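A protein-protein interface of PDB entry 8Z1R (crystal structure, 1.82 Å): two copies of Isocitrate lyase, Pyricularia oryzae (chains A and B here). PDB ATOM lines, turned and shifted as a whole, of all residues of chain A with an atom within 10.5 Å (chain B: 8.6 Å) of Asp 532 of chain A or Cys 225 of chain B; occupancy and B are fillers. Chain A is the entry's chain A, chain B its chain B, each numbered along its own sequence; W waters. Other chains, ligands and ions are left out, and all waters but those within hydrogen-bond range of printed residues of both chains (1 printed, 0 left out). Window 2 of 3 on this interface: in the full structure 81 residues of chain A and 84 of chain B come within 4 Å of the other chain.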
ATOM      1  N   MET A 155     -32.683  -7.628 -18.064  1.00  0.00           N
ATOM      2  CA  MET A 155     -31.454  -8.363 -17.773  1.00  0.00           C
ATOM      3  C   MET A 155     -31.748  -9.799 -17.339  1.00  0.00           C
ATOM      4  O   MET A 155     -31.129 -10.747 -17.839  1.00  0.00           O
ATOM      5  CB  MET A 155     -30.657  -7.614 -16.701  1.00  0.00           C
ATOM      6  CG  MET A 155     -29.533  -8.393 -16.006  1.00  0.00           C
ATOM      7  SD  MET A 155     -28.040  -8.526 -16.990  1.00  0.00           S
ATOM      8  CE  MET A 155     -28.093  -7.045 -18.006  1.00  0.00           C
ATOM      9  N   LYS A 159     -30.781 -13.330 -19.129  1.00  0.00           N
ATOM     10  CA  LYS A 159     -30.082 -14.401 -18.424  1.00  0.00           C
ATOM     11  C   LYS A 159     -30.874 -15.703 -18.486  1.00  0.00           C
ATOM     12  O   LYS A 159     -30.313 -16.778 -18.734  1.00  0.00           O
ATOM     13  CB  LYS A 159     -29.845 -13.980 -16.973  1.00  0.00           C
ATOM     14  CG  LYS A 159     -29.362 -15.086 -16.062  1.00  0.00           C
ATOM     15  CD  LYS A 159     -29.522 -14.705 -14.592  1.00  0.00           C
ATOM     16  CE  LYS A 159     -30.985 -14.754 -14.168  1.00  0.00           C
ATOM     17  NZ  LYS A 159     -31.156 -14.580 -12.693  1.00  0.00           N
ATOM     18  N   ASP A 162     -30.902 -17.237 -22.033  1.00  0.00           N
ATOM     19  CA  ASP A 162     -29.579 -17.808 -22.277  1.00  0.00           C
ATOM     20  C   ASP A 162     -29.404 -19.138 -21.548  1.00  0.00           C
ATOM     21  O   ASP A 162     -28.859 -20.095 -22.109  1.00  0.00           O
ATOM     22  CB  ASP A 162     -28.503 -16.816 -21.839  1.00  0.00           C
ATOM     23  CG  ASP A 162     -27.111 -17.402 -21.882  1.00  0.00           C
ATOM     24  OD1 ASP A 162     -26.545 -17.506 -22.990  1.00  0.00           O
ATOM     25  OD2 ASP A 162     -26.586 -17.753 -20.804  1.00  0.00           O
ATOM     26  N   LYS A 166     -28.952 -23.272 -23.221  1.00  0.00           N
ATOM     27  CA  LYS A 166     -27.902 -24.210 -22.840  1.00  0.00           C
ATOM     28  C   LYS A 166     -28.441 -25.551 -22.355  1.00  0.00           C
ATOM     29  O   LYS A 166     -27.647 -26.468 -22.121  1.00  0.00           O
ATOM     30  CB  LYS A 166     -27.018 -23.595 -21.750  1.00  0.00           C
ATOM     31  CG  LYS A 166     -25.628 -23.198 -22.213  1.00  0.00           C
ATOM     32  CD  LYS A 166     -25.687 -22.063 -23.217  1.00  0.00           C
ATOM     33  CE  LYS A 166     -25.466 -22.528 -24.652  1.00  0.00           C
ATOM     34  NZ  LYS A 166     -25.595 -21.397 -25.621  1.00  0.00           N
ATOM     35  N   GLN A 523     -23.391 -15.268  -7.751  1.00  0.00           N
ATOM     36  CA  GLN A 523     -22.737 -15.022  -9.033  1.00  0.00           C
ATOM     37  C   GLN A 523     -23.633 -15.444 -10.190  1.00  0.00           C
ATOM     38  O   GLN A 523     -23.883 -14.663 -11.118  1.00  0.00           O
ATOM     39  CB  GLN A 523     -21.394 -15.755  -9.093  1.00  0.00           C
ATOM     40  CG  GLN A 523     -20.257 -15.021  -8.405  1.00  0.00           C
ATOM     41  CD  GLN A 523     -19.946 -13.688  -9.067  1.00  0.00           C
ATOM     42  OE1 GLN A 523     -20.475 -12.647  -8.670  1.00  0.00           O
ATOM     43  NE2 GLN A 523     -19.088 -13.715 -10.086  1.00  0.00           N
ATOM     44  N   LYS A 524     -24.131 -16.686 -10.145  1.00  0.00           N
ATOM     45  CA  LYS A 524     -25.043 -17.162 -11.177  1.00  0.00           C
ATOM     46  C   LYS A 524     -26.336 -16.353 -11.181  1.00  0.00           C
ATOM     47  O   LYS A 524     -26.849 -16.000 -12.249  1.00  0.00           O
ATOM     48  CB  LYS A 524     -25.341 -18.647 -10.968  1.00  0.00           C
ATOM     49  CG  LYS A 524     -26.307 -19.233 -11.989  1.00  0.00           C
ATOM     50  CD  LYS A 524     -26.511 -20.725 -11.762  1.00  0.00           C
ATOM     51  CE  LYS A 524     -27.026 -21.015 -10.359  1.00  0.00           C
ATOM     52  NZ  LYS A 524     -28.483 -21.357 -10.328  1.00  0.00           N
ATOM     53  N   SER A 526     -26.788 -13.275 -10.499  1.00  0.00           N
ATOM     54  CA  SER A 526     -26.586 -11.955 -11.091  1.00  0.00           C
ATOM     55  C   SER A 526     -26.438 -12.004 -12.607  1.00  0.00           C
ATOM     56  O   SER A 526     -26.513 -10.955 -13.254  1.00  0.00           O
ATOM     57  CB  SER A 526     -25.351 -11.285 -10.481  1.00  0.00           C
ATOM     58  OG  SER A 526     -24.155 -11.921 -10.926  1.00  0.00           O
ATOM     59  N   GLY A 527     -26.213 -13.179 -13.179  1.00  0.00           N
ATOM     60  CA  GLY A 527     -26.039 -13.337 -14.608  1.00  0.00           C
ATOM     61  C   GLY A 527     -24.602 -13.549 -15.089  1.00  0.00           C
ATOM     62  O   GLY A 527     -24.327 -13.299 -16.271  1.00  0.00           O
ATOM     63  N   ALA A 528     -23.693 -13.993 -14.214  1.00  0.00           N
ATOM     64  CA  ALA A 528     -22.281 -14.093 -14.578  1.00  0.00           C
ATOM     65  C   ALA A 528     -22.068 -15.002 -15.785  1.00  0.00           C
ATOM     66  O   ALA A 528     -21.266 -14.688 -16.672  1.00  0.00           O
ATOM     67  CB  ALA A 528     -21.469 -14.594 -13.383  1.00  0.00           C
ATOM     68  N   ALA A 529     -22.772 -16.137 -15.840  1.00  0.00           N
ATOM     69  CA  ALA A 529     -22.585 -17.051 -16.965  1.00  0.00           C
ATOM     70  C   ALA A 529     -23.009 -16.398 -18.276  1.00  0.00           C
ATOM     71  O   ALA A 529     -22.393 -16.628 -19.325  1.00  0.00           O
ATOM     72  CB  ALA A 529     -23.361 -18.349 -16.731  1.00  0.00           C
ATOM     73  N   TYR A 530     -24.057 -15.569 -18.224  1.00  0.00           N
ATOM     74  CA  TYR A 530     -24.533 -14.865 -19.410  1.00  0.00           C
ATOM     75  C   TYR A 530     -23.445 -13.972 -19.995  1.00  0.00           C
ATOM     76  O   TYR A 530     -23.139 -14.043 -21.194  1.00  0.00           O
ATOM     77  CB  TYR A 530     -25.773 -14.047 -19.042  1.00  0.00           C
ATOM     78  CG  TYR A 530     -26.287 -13.120 -20.121  1.00  0.00           C
ATOM     79  CD1 TYR A 530     -27.175 -13.573 -21.087  1.00  0.00           C
ATOM     80  CD2 TYR A 530     -25.912 -11.781 -20.152  1.00  0.00           C
ATOM     81  CE1 TYR A 530     -27.661 -12.727 -22.072  1.00  0.00           C
ATOM     82  CE2 TYR A 530     -26.394 -10.923 -21.132  1.00  0.00           C
ATOM     83  CZ  TYR A 530     -27.269 -11.403 -22.090  1.00  0.00           C
ATOM     84  OH  TYR A 530     -27.753 -10.554 -23.066  1.00  0.00           O
ATOM     85  N   MET A 531     -22.846 -13.119 -19.158  1.00  0.00           N
ATOM     86  CA  MET A 531     -21.791 -12.235 -19.639  1.00  0.00           C
ATOM     87  C   MET A 531     -20.558 -13.013 -20.075  1.00  0.00           C
ATOM     88  O   MET A 531     -19.876 -12.605 -21.020  1.00  0.00           O
ATOM     89  CB  MET A 531     -21.411 -11.217 -18.562  1.00  0.00           C
ATOM     90  CG  MET A 531     -22.342 -10.015 -18.477  1.00  0.00           C
ATOM     91  SD  MET A 531     -22.402  -9.013 -19.989  1.00  0.00           S
ATOM     92  CE  MET A 531     -20.710  -9.053 -20.535  1.00  0.00           C
ATOM     93  N   ASP A 532     -20.261 -14.133 -19.407  1.00  0.00           N
ATOM     94  CA  ASP A 532     -19.107 -14.941 -19.794  1.00  0.00           C
ATOM     95  C   ASP A 532     -19.208 -15.403 -21.242  1.00  0.00           C
ATOM     96  O   ASP A 532     -18.223 -15.345 -21.988  1.00  0.00           O
ATOM     97  CB  ASP A 532     -18.967 -16.143 -18.862  1.00  0.00           C
ATOM     98  CG  ASP A 532     -18.416 -15.761 -17.511  1.00  0.00           C
ATOM     99  OD1 ASP A 532     -18.100 -14.564 -17.323  1.00  0.00           O
ATOM    100  OD2 ASP A 532     -18.296 -16.652 -16.642  1.00  0.00           O
ATOM    101  N   ARG A 533     -20.395 -15.856 -21.658  1.00  0.00           N
ATOM    102  CA  ARG A 533     -20.568 -16.347 -23.023  1.00  0.00           C
ATOM    103  C   ARG A 533     -20.401 -15.229 -24.045  1.00  0.00           C
ATOM    104  O   ARG A 533     -19.798 -15.435 -25.104  1.00  0.00           O
ATOM    105  CB  ARG A 533     -21.941 -16.999 -23.179  1.00  0.00           C
ATOM    106  CG  ARG A 533     -22.101 -18.325 -22.451  1.00  0.00           C
ATOM    107  CD  ARG A 533     -23.545 -18.823 -22.540  1.00  0.00           C
ATOM    108  NE  ARG A 533     -23.774 -20.005 -21.718  1.00  0.00           N
ATOM    109  CZ  ARG A 533     -24.294 -19.991 -20.496  1.00  0.00           C
ATOM    110  NH1 ARG A 533     -24.639 -18.860 -19.905  1.00  0.00           N
ATOM    111  NH2 ARG A 533     -24.475 -21.141 -19.853  1.00  0.00           N
ATOM    112  N   ILE A 534     -20.946 -14.044 -23.754  1.00  0.00           N
ATOM    113  CA  ILE A 534     -20.840 -12.924 -24.690  1.00  0.00           C
ATOM    114  C   ILE A 534     -19.380 -12.541 -24.899  1.00  0.00           C
ATOM    115  O   ILE A 534     -18.922 -12.361 -26.036  1.00  0.00           O
ATOM    116  CB  ILE A 534     -21.672 -11.732 -24.190  1.00  0.00           C
ATOM    117  CG1 ILE A 534     -23.159 -12.089 -24.238  1.00  0.00           C
ATOM    118  CG2 ILE A 534     -21.381 -10.488 -25.018  1.00  0.00           C
ATOM    119  CD1 ILE A 534     -24.056 -11.005 -23.708  1.00  0.00           C
ATOM    120  N   VAL A 535     -18.626 -12.409 -23.803  1.00  0.00           N
ATOM    121  CA  VAL A 535     -17.210 -12.070 -23.918  1.00  0.00           C
ATOM    122  C   VAL A 535     -16.463 -13.166 -24.672  1.00  0.00           C
ATOM    123  O   VAL A 535     -15.613 -12.885 -25.527  1.00  0.00           O
ATOM    124  CB  VAL A 535     -16.601 -11.823 -22.524  1.00  0.00           C
ATOM    125  CG1 VAL A 535     -15.144 -11.415 -22.651  1.00  0.00           C
ATOM    126  CG2 VAL A 535     -17.390 -10.759 -21.778  1.00  0.00           C
ATOM    127  N   GLY A 536     -16.775 -14.432 -24.374  1.00  0.00           N
ATOM    128  CA  GLY A 536     -16.149 -15.528 -25.102  1.00  0.00           C
ATOM    129  C   GLY A 536     -16.444 -15.499 -26.591  1.00  0.00           C
ATOM    130  O   GLY A 536     -15.586 -15.845 -27.410  1.00  0.00           O
ATOM    131  N   ALA A 537     -17.660 -15.082 -26.963  1.00  0.00           N
ATOM    132  CA  ALA A 537     -18.002 -14.961 -28.379  1.00  0.00           C
ATOM    133  C   ALA A 537     -17.210 -13.843 -29.055  1.00  0.00           C
ATOM    134  O   ALA A 537     -16.819 -13.970 -30.223  1.00  0.00           O
ATOM    135  CB  ALA A 537     -19.506 -14.725 -28.541  1.00  0.00           C
ATOM    136  N   ILE A 538     -16.962 -12.740 -28.342  1.00  0.00           N
ATOM    137  CA  ILE A 538     -16.269 -11.604 -28.952  1.00  0.00           C
ATOM    138  C   ILE A 538     -14.811 -11.951 -29.244  1.00  0.00           C
ATOM    139  O   ILE A 538     -14.268 -11.585 -30.296  1.00  0.00           O
ATOM    140  CB  ILE A 538     -16.393 -10.360 -28.052  1.00  0.00           C
ATOM    141  CG1 ILE A 538     -17.850  -9.883 -28.032  1.00  0.00           C
ATOM    142  CG2 ILE A 538     -15.429  -9.255 -28.523  1.00  0.00           C
ATOM    143  CD1 ILE A 538     -18.205  -9.000 -26.871  1.00  0.00           C
ATOM    144  N   GLN A 539     -14.164 -12.673 -28.335  1.00  0.00           N
ATOM    145  CA  GLN A 539     -12.742 -12.987 -28.470  1.00  0.00           C
ATOM    146  C   GLN A 539     -12.484 -14.183 -29.387  1.00  0.00           C
ATOM    147  O   GLN A 539     -13.134 -15.225 -29.275  1.00  0.00           O
ATOM    148  CB  GLN A 539     -12.140 -13.245 -27.085  1.00  0.00           C
ATOM    149  CG  GLN A 539     -12.372 -12.096 -26.112  1.00  0.00           C
ATOM    150  CD  GLN A 539     -11.837 -12.379 -24.721  1.00  0.00           C
ATOM    151  OE1 GLN A 539     -12.088 -13.440 -24.148  1.00  0.00           O
ATOM    152  NE2 GLN A 539     -11.091 -11.427 -24.170  1.00  0.00           N
ATOM    153  N   PRO B 132     -23.953  -8.501 -14.044  1.00  0.00           N
ATOM    154  CA  PRO B 132     -22.954  -9.105 -13.151  1.00  0.00           C
ATOM    155  C   PRO B 132     -21.800  -8.144 -12.900  1.00  0.00           C
ATOM    156  O   PRO B 132     -21.500  -7.263 -13.709  1.00  0.00           O
ATOM    157  CB  PRO B 132     -22.471 -10.343 -13.914  1.00  0.00           C
ATOM    158  CG  PRO B 132     -23.402 -10.529 -15.034  1.00  0.00           C
ATOM    159  CD  PRO B 132     -24.099  -9.250 -15.305  1.00  0.00           C
ATOM    160  N   ASP B 133     -21.129  -8.347 -11.765  1.00  0.00           N
ATOM    161  CA  ASP B 133     -20.079  -7.440 -11.312  1.00  0.00           C
ATOM    162  C   ASP B 133     -18.805  -7.669 -12.117  1.00  0.00           C
ATOM    163  O   ASP B 133     -18.101  -8.664 -11.915  1.00  0.00           O
ATOM    164  CB  ASP B 133     -19.820  -7.632  -9.822  1.00  0.00           C
ATOM    165  CG  ASP B 133     -18.797  -6.646  -9.274  1.00  0.00           C
ATOM    166  OD1 ASP B 133     -18.603  -5.572  -9.888  1.00  0.00           O
ATOM    167  OD2 ASP B 133     -18.178  -6.953  -8.234  1.00  0.00           O
ATOM    168  N   PHE B 134     -18.513  -6.741 -13.028  1.00  0.00           N
ATOM    169  CA  PHE B 134     -17.218  -6.645 -13.690  1.00  0.00           C
ATOM    170  C   PHE B 134     -16.548  -5.304 -13.401  1.00  0.00           C
ATOM    171  O   PHE B 134     -15.575  -4.944 -14.080  1.00  0.00           O
ATOM    172  CB  PHE B 134     -17.366  -6.836 -15.206  1.00  0.00           C
ATOM    173  CG  PHE B 134     -17.676  -8.258 -15.632  1.00  0.00           C
ATOM    174  CD1 PHE B 134     -18.846  -8.888 -15.232  1.00  0.00           C
ATOM    175  CD2 PHE B 134     -16.809  -8.945 -16.468  1.00  0.00           C
ATOM    176  CE1 PHE B 134     -19.134 -10.189 -15.633  1.00  0.00           C
ATOM    177  CE2 PHE B 134     -17.092 -10.248 -16.877  1.00  0.00           C
ATOM    178  CZ  PHE B 134     -18.258 -10.867 -16.459  1.00  0.00           C
ATOM    179  N   GLY B 221     -10.979  -3.293 -16.370  1.00  0.00           N
ATOM    180  CA  GLY B 221     -11.435  -3.993 -17.545  1.00  0.00           C
ATOM    181  C   GLY B 221     -11.818  -5.407 -17.244  1.00  0.00           C
ATOM    182  O   GLY B 221     -12.244  -6.129 -18.152  1.00  0.00           O
ATOM    183  N   GLY B 222     -11.655  -5.834 -16.001  1.00  0.00           N
ATOM    184  CA  GLY B 222     -12.239  -7.070 -15.540  1.00  0.00           C
ATOM    185  C   GLY B 222     -11.372  -8.290 -15.743  1.00  0.00           C
ATOM    186  O   GLY B 222     -10.253  -8.257 -16.273  1.00  0.00           O
ATOM    187  N   LYS B 223     -11.945  -9.406 -15.315  1.00  0.00           N
ATOM    188  CA  LYS B 223     -11.259 -10.681 -15.322  1.00  0.00           C
ATOM    189  C   LYS B 223     -11.206 -11.270 -16.730  1.00  0.00           C
ATOM    190  O   LYS B 223     -12.024 -10.945 -17.598  1.00  0.00           O
ATOM    191  CB  LYS B 223     -11.990 -11.640 -14.371  1.00  0.00           C
ATOM    192  CG  LYS B 223     -12.295 -11.005 -13.009  1.00  0.00           C
ATOM    193  CD  LYS B 223     -13.109 -11.938 -12.115  1.00  0.00           C
ATOM    194  CE  LYS B 223     -12.424 -13.283 -11.964  1.00  0.00           C
ATOM    195  NZ  LYS B 223     -13.171 -14.219 -11.074  1.00  0.00           N
ATOM    196  N   LYS B 224     -10.210 -12.122 -16.961  1.00  0.00           N
ATOM    197  CA  LYS B 224     -10.211 -12.950 -18.155  1.00  0.00           C
ATOM    198  C   LYS B 224     -11.327 -13.986 -18.045  1.00  0.00           C
ATOM    199  O   LYS B 224     -11.674 -14.441 -16.950  1.00  0.00           O
ATOM    200  CB  LYS B 224      -8.851 -13.634 -18.337  1.00  0.00           C
ATOM    201  CG  LYS B 224      -8.638 -14.300 -19.698  1.00  0.00           C
ATOM    202  CD  LYS B 224      -7.376 -15.162 -19.712  1.00  0.00           C
ATOM    203  CE  LYS B 224      -7.064 -15.696 -21.105  1.00  0.00           C
ATOM    204  NZ  LYS B 224      -8.246 -16.328 -21.751  1.00  0.00           N
ATOM    205  N   CYS B 225     -11.914 -14.340 -19.186  1.00  0.00           N
ATOM    206  CA  CYS B 225     -12.985 -15.325 -19.216  1.00  0.00           C
ATOM    207  C   CYS B 225     -12.601 -16.504 -20.104  1.00  0.00           C
ATOM    208  O   CYS B 225     -11.774 -16.385 -21.014  1.00  0.00           O
ATOM    209  CB  CYS B 225     -14.303 -14.705 -19.712  1.00  0.00           C
ATOM    210  SG  CYS B 225     -14.959 -13.372 -18.665  1.00  0.00           S
ATOM    211  N   GLY B 226     -13.207 -17.648 -19.820  1.00  0.00           N
ATOM    212  CA  GLY B 226     -13.004 -18.854 -20.622  1.00  0.00           C
ATOM    213  C   GLY B 226     -11.842 -19.690 -20.095  1.00  0.00           C
ATOM    214  O   GLY B 226     -11.854 -20.111 -18.939  1.00  0.00           O
ATOM    215  N   HIS B 227     -10.852 -19.926 -20.952  1.00  0.00           N
ATOM    216  CA  HIS B 227      -9.676 -20.694 -20.562  1.00  0.00           C
ATOM    217  C   HIS B 227      -8.770 -19.852 -19.670  1.00  0.00           C
ATOM    218  O   HIS B 227      -8.420 -18.719 -20.017  1.00  0.00           O
ATOM    219  CB  HIS B 227      -8.925 -21.166 -21.806  1.00  0.00           C
ATOM    220  CG  HIS B 227      -7.576 -21.749 -21.520  1.00  0.00           C
ATOM    221  ND1 HIS B 227      -6.403 -21.079 -21.797  1.00  0.00           N
ATOM    222  CD2 HIS B 227      -7.213 -22.940 -20.986  1.00  0.00           C
ATOM    223  CE1 HIS B 227      -5.376 -21.832 -21.444  1.00  0.00           C
ATOM    224  NE2 HIS B 227      -5.840 -22.966 -20.949  1.00  0.00           N
ATOM    225  N   LEU B 228      -8.391 -20.415 -18.520  1.00  0.00           N
ATOM    226  CA  LEU B 228      -7.637 -19.693 -17.492  1.00  0.00           C
ATOM    227  C   LEU B 228      -8.407 -18.466 -17.007  1.00  0.00           C
ATOM    228  O   LEU B 228      -7.825 -17.418 -16.715  1.00  0.00           O
ATOM    229  CB  LEU B 228      -6.240 -19.305 -17.984  1.00  0.00           C
ATOM    230  CG  LEU B 228      -5.273 -20.452 -18.278  1.00  0.00           C
ATOM    231  CD1 LEU B 228      -4.001 -19.914 -18.912  1.00  0.00           C
ATOM    232  CD2 LEU B 228      -4.954 -21.249 -17.016  1.00  0.00           C
ATOM    233  N   ALA B 229      -9.730 -18.599 -16.927  1.00  0.00           N
ATOM    234  CA  ALA B 229     -10.562 -17.516 -16.422  1.00  0.00           C
ATOM    235  C   ALA B 229     -10.159 -17.170 -14.995  1.00  0.00           C
ATOM    236  O   ALA B 229      -9.832 -18.049 -14.192  1.00  0.00           O
ATOM    237  CB  ALA B 229     -12.037 -17.910 -16.477  1.00  0.00           C
ATOM    238  N   GLY B 230     -10.159 -15.880 -14.686  1.00  0.00           N
ATOM    239  CA  GLY B 230      -9.814 -15.437 -13.354  1.00  0.00           C
ATOM    240  C   GLY B 230      -9.353 -13.990 -13.356  1.00  0.00           C
ATOM    241  O   GLY B 230      -9.342 -13.315 -14.385  1.00  0.00           O
ATOM    242  N   LYS B 231      -8.954 -13.548 -12.171  1.00  0.00           N
ATOM    243  CA  LYS B 231      -8.536 -12.173 -11.960  1.00  0.00           C
ATOM    244  C   LYS B 231      -7.205 -11.878 -12.654  1.00  0.00           C
ATOM    245  O   LYS B 231      -6.367 -12.765 -12.853  1.00  0.00           O
ATOM    246  CB  LYS B 231      -8.409 -11.895 -10.462  1.00  0.00           C
ATOM    247  CG  LYS B 231      -9.700 -12.086  -9.679  1.00  0.00           C
ATOM    248  CD  LYS B 231      -9.416 -12.262  -8.197  1.00  0.00           C
ATOM    249  CE  LYS B 231     -10.704 -12.329  -7.403  1.00  0.00           C
ATOM    250  NZ  LYS B 231     -10.431 -12.622  -5.966  1.00  0.00           N
ATOM    251  N   VAL B 232      -7.010 -10.610 -13.004  1.00  0.00           N
ATOM    252  CA  VAL B 232      -5.749 -10.122 -13.566  1.00  0.00           C
ATOM    253  C   VAL B 232      -5.227  -9.025 -12.644  1.00  0.00           C
ATOM    254  O   VAL B 232      -5.922  -8.030 -12.405  1.00  0.00           O
ATOM    255  CB  VAL B 232      -5.916  -9.590 -14.998  1.00  0.00           C
ATOM    256  CG1 VAL B 232      -4.554  -9.181 -15.565  1.00  0.00           C
ATOM    257  CG2 VAL B 232      -6.584 -10.634 -15.879  1.00  0.00           C
ATOM    258  N   LEU B 270      -2.758 -14.226 -13.026  1.00  0.00           N
ATOM    259  CA  LEU B 270      -2.312 -13.500 -14.209  1.00  0.00           C
ATOM    260  C   LEU B 270      -1.936 -12.092 -13.786  1.00  0.00           C
ATOM    261  O   LEU B 270      -2.538 -11.539 -12.863  1.00  0.00           O
ATOM    262  CB  LEU B 270      -3.408 -13.441 -15.281  1.00  0.00           C
ATOM    263  CG  LEU B 270      -3.858 -14.793 -15.844  1.00  0.00           C
ATOM    264  CD1 LEU B 270      -5.203 -14.668 -16.555  1.00  0.00           C
ATOM    265  CD2 LEU B 270      -2.787 -15.357 -16.802  1.00  0.00           C
ATOM    266  N   ASP B 312      -8.873 -23.449 -29.434  1.00  0.00           N
ATOM    267  CA  ASP B 312      -9.013 -23.925 -28.061  1.00  0.00           C
ATOM    268  C   ASP B 312      -8.196 -25.188 -27.824  1.00  0.00           C
ATOM    269  O   ASP B 312      -7.603 -25.361 -26.753  1.00  0.00           O
ATOM    270  CB  ASP B 312     -10.488 -24.181 -27.749  1.00  0.00           C
ATOM    271  CG  ASP B 312     -11.178 -22.973 -27.147  1.00  0.00           C
ATOM    272  OD1 ASP B 312     -10.963 -22.704 -25.946  1.00  0.00           O
ATOM    273  OD2 ASP B 312     -11.929 -22.286 -27.873  1.00  0.00           O
ATOM    274  N   GLU B 315      -4.280 -24.424 -27.687  1.00  0.00           N
ATOM    275  CA  GLU B 315      -3.940 -23.780 -26.426  1.00  0.00           C
ATOM    276  C   GLU B 315      -3.906 -24.794 -25.289  1.00  0.00           C
ATOM    277  O   GLU B 315      -2.936 -24.857 -24.526  1.00  0.00           O
ATOM    278  CB  GLU B 315      -4.930 -22.658 -26.119  1.00  0.00           C
ATOM    279  CG  GLU B 315      -4.738 -22.088 -24.730  1.00  0.00           C
ATOM    280  CD  GLU B 315      -5.087 -20.620 -24.639  1.00  0.00           C
ATOM    281  OE1 GLU B 315      -5.855 -20.137 -25.497  1.00  0.00           O
ATOM    282  OE2 GLU B 315      -4.586 -19.949 -23.708  1.00  0.00           O
ATOM    283  N   GLU B 386      -4.347 -12.060 -24.664  1.00  0.00           N
ATOM    284  CA  GLU B 386      -4.382 -10.648 -24.321  1.00  0.00           C
ATOM    285  C   GLU B 386      -2.997 -10.096 -24.035  1.00  0.00           C
ATOM    286  O   GLU B 386      -2.833  -8.872 -23.969  1.00  0.00           O
ATOM    287  CB  GLU B 386      -5.282 -10.414 -23.100  1.00  0.00           C
ATOM    288  CG  GLU B 386      -6.724 -10.881 -23.272  1.00  0.00           C
ATOM    289  CD  GLU B 386      -6.913 -12.359 -22.940  1.00  0.00           C
ATOM    290  OE1 GLU B 386      -5.913 -13.055 -22.627  1.00  0.00           O
ATOM    291  OE2 GLU B 386      -8.067 -12.822 -22.983  1.00  0.00           O
ATOM    292  N   TYR B 388      -1.240 -11.290 -21.241  1.00  0.00           N
ATOM    293  CA  TYR B 388      -1.034 -11.348 -19.801  1.00  0.00           C
ATOM    294  C   TYR B 388       0.043 -12.368 -19.467  1.00  0.00           C
ATOM    295  O   TYR B 388       0.206 -13.361 -20.173  1.00  0.00           O
ATOM    296  CB  TYR B 388      -2.315 -11.731 -19.072  1.00  0.00           C
ATOM    297  CG  TYR B 388      -3.468 -10.798 -19.351  1.00  0.00           C
ATOM    298  CD1 TYR B 388      -3.263  -9.443 -19.593  1.00  0.00           C
ATOM    299  CD2 TYR B 388      -4.771 -11.284 -19.387  1.00  0.00           C
ATOM    300  CE1 TYR B 388      -4.357  -8.597 -19.856  1.00  0.00           C
ATOM    301  CE2 TYR B 388      -5.834 -10.462 -19.640  1.00  0.00           C
ATOM    302  CZ  TYR B 388      -5.623  -9.130 -19.875  1.00  0.00           C
ATOM    303  OH  TYR B 388      -6.730  -8.344 -20.111  1.00  0.00           O
HETATM  304  O   HOH W   1     -21.886 -10.636 -10.320  1.00  0.00           O
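OD1 of Asp 532 of chain A sits at hydrogen-bond distance from SG of Cys 225 of chain B, at 3.6 Å.
The backbone carbonyl oxygen (O) of Gln 523 of chain A is in hydrogen-bond range of the side-chain hydroxyl (OG) of Ser 526 of chain A. The backbone NH of Ala 528 of chain A is in hydrogen-bond range of the backbone carbonyl oxygen of Gln 523 of chain A. OE2 of Glu 386 of chain B lies within salt-bridge range of NZ of Lys 224 of chain B (3.7 Å).
Ser 526 of chain A touches Pro 132 of chain B. Gly 527 of chain A touches Pro 132 of chain B (O to CG, 3.2 Å). Ala 528 of chain A touches Pro 132 of chain B. Met 531 of chain A touches Pro 132 of chain B (CG to CG, 3.6 Å). CB of Met 531 of chain A touches CZ of Phe 134 of chain B, 3.8 Å away. CZ of Phe 134 of chain B touches OD1 of Asp 532 of chain A (3.8 Å). Gln 539 of chain A touches Glu 386 of chain B (NE2 to OE2, 3.5 Å).
Lys 524 of chain A touches none of the printed residues of chain B. Printed residues of chain B within 4 Å of Ser 526 of chain A: Pro 132. Of the printed residues of chain B, Ala 528 of chain A touches Pro 132 (3.6 Å). Of chain B, only Phe 134 and Cys 225 come within 4 Å of Asp 532 of chain A. Printed residues of chain B within 4 Å of Gln 539 of chain A: Glu 386 (3.5 Å). Printed residues of chain A within 4 Å of Pro 132 of chain B: Ser 526 (3.6 Å), Gly 527 (3.2 Å), Ala 528 (3.6 Å) and Met 531 (3.6 Å). Printed residues of chain A within 4 Å of Phe 134 of chain B: Met 531 and Asp 532. No residue of chain A comes within 4 Å of Gly 226 of chain B. The nearest residue of chain A that does not touch Cys 225 of chain B is Gln 539 of chain A (4.3 Å). The nearest printed residue of chain B that does not touch Ser 526 of chain A is Asp 133 of chain B (4.8 Å).
Of the 20 printed residues of chain B, 4 touch a printed residue of chain A. Of the 20 printed residues of chain A, 6 touch a printed residue of chain B. Hydrophobic or aromatic side chains of chain A that line the printed part of chain B: Met 531. Among the printed residues, 8 pairs touch across the chains. Among the printed residues, no Asp or Glu carboxylate lies within 4 Å of a Lys or Arg side-chain nitrogen of the other chain.
No position is printed for both chains. Of the 8 pairs that touch across the chains among the printed residues, none has its exchanged pair printed and touching as well.
Water W1 lies within hydrogen-bond range of the side-chain hydroxyl of Ser 526 of chain A, the backbone NH of Asp 133 of chain B and the side-chain amide oxygen of Gln 523 of chain A.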
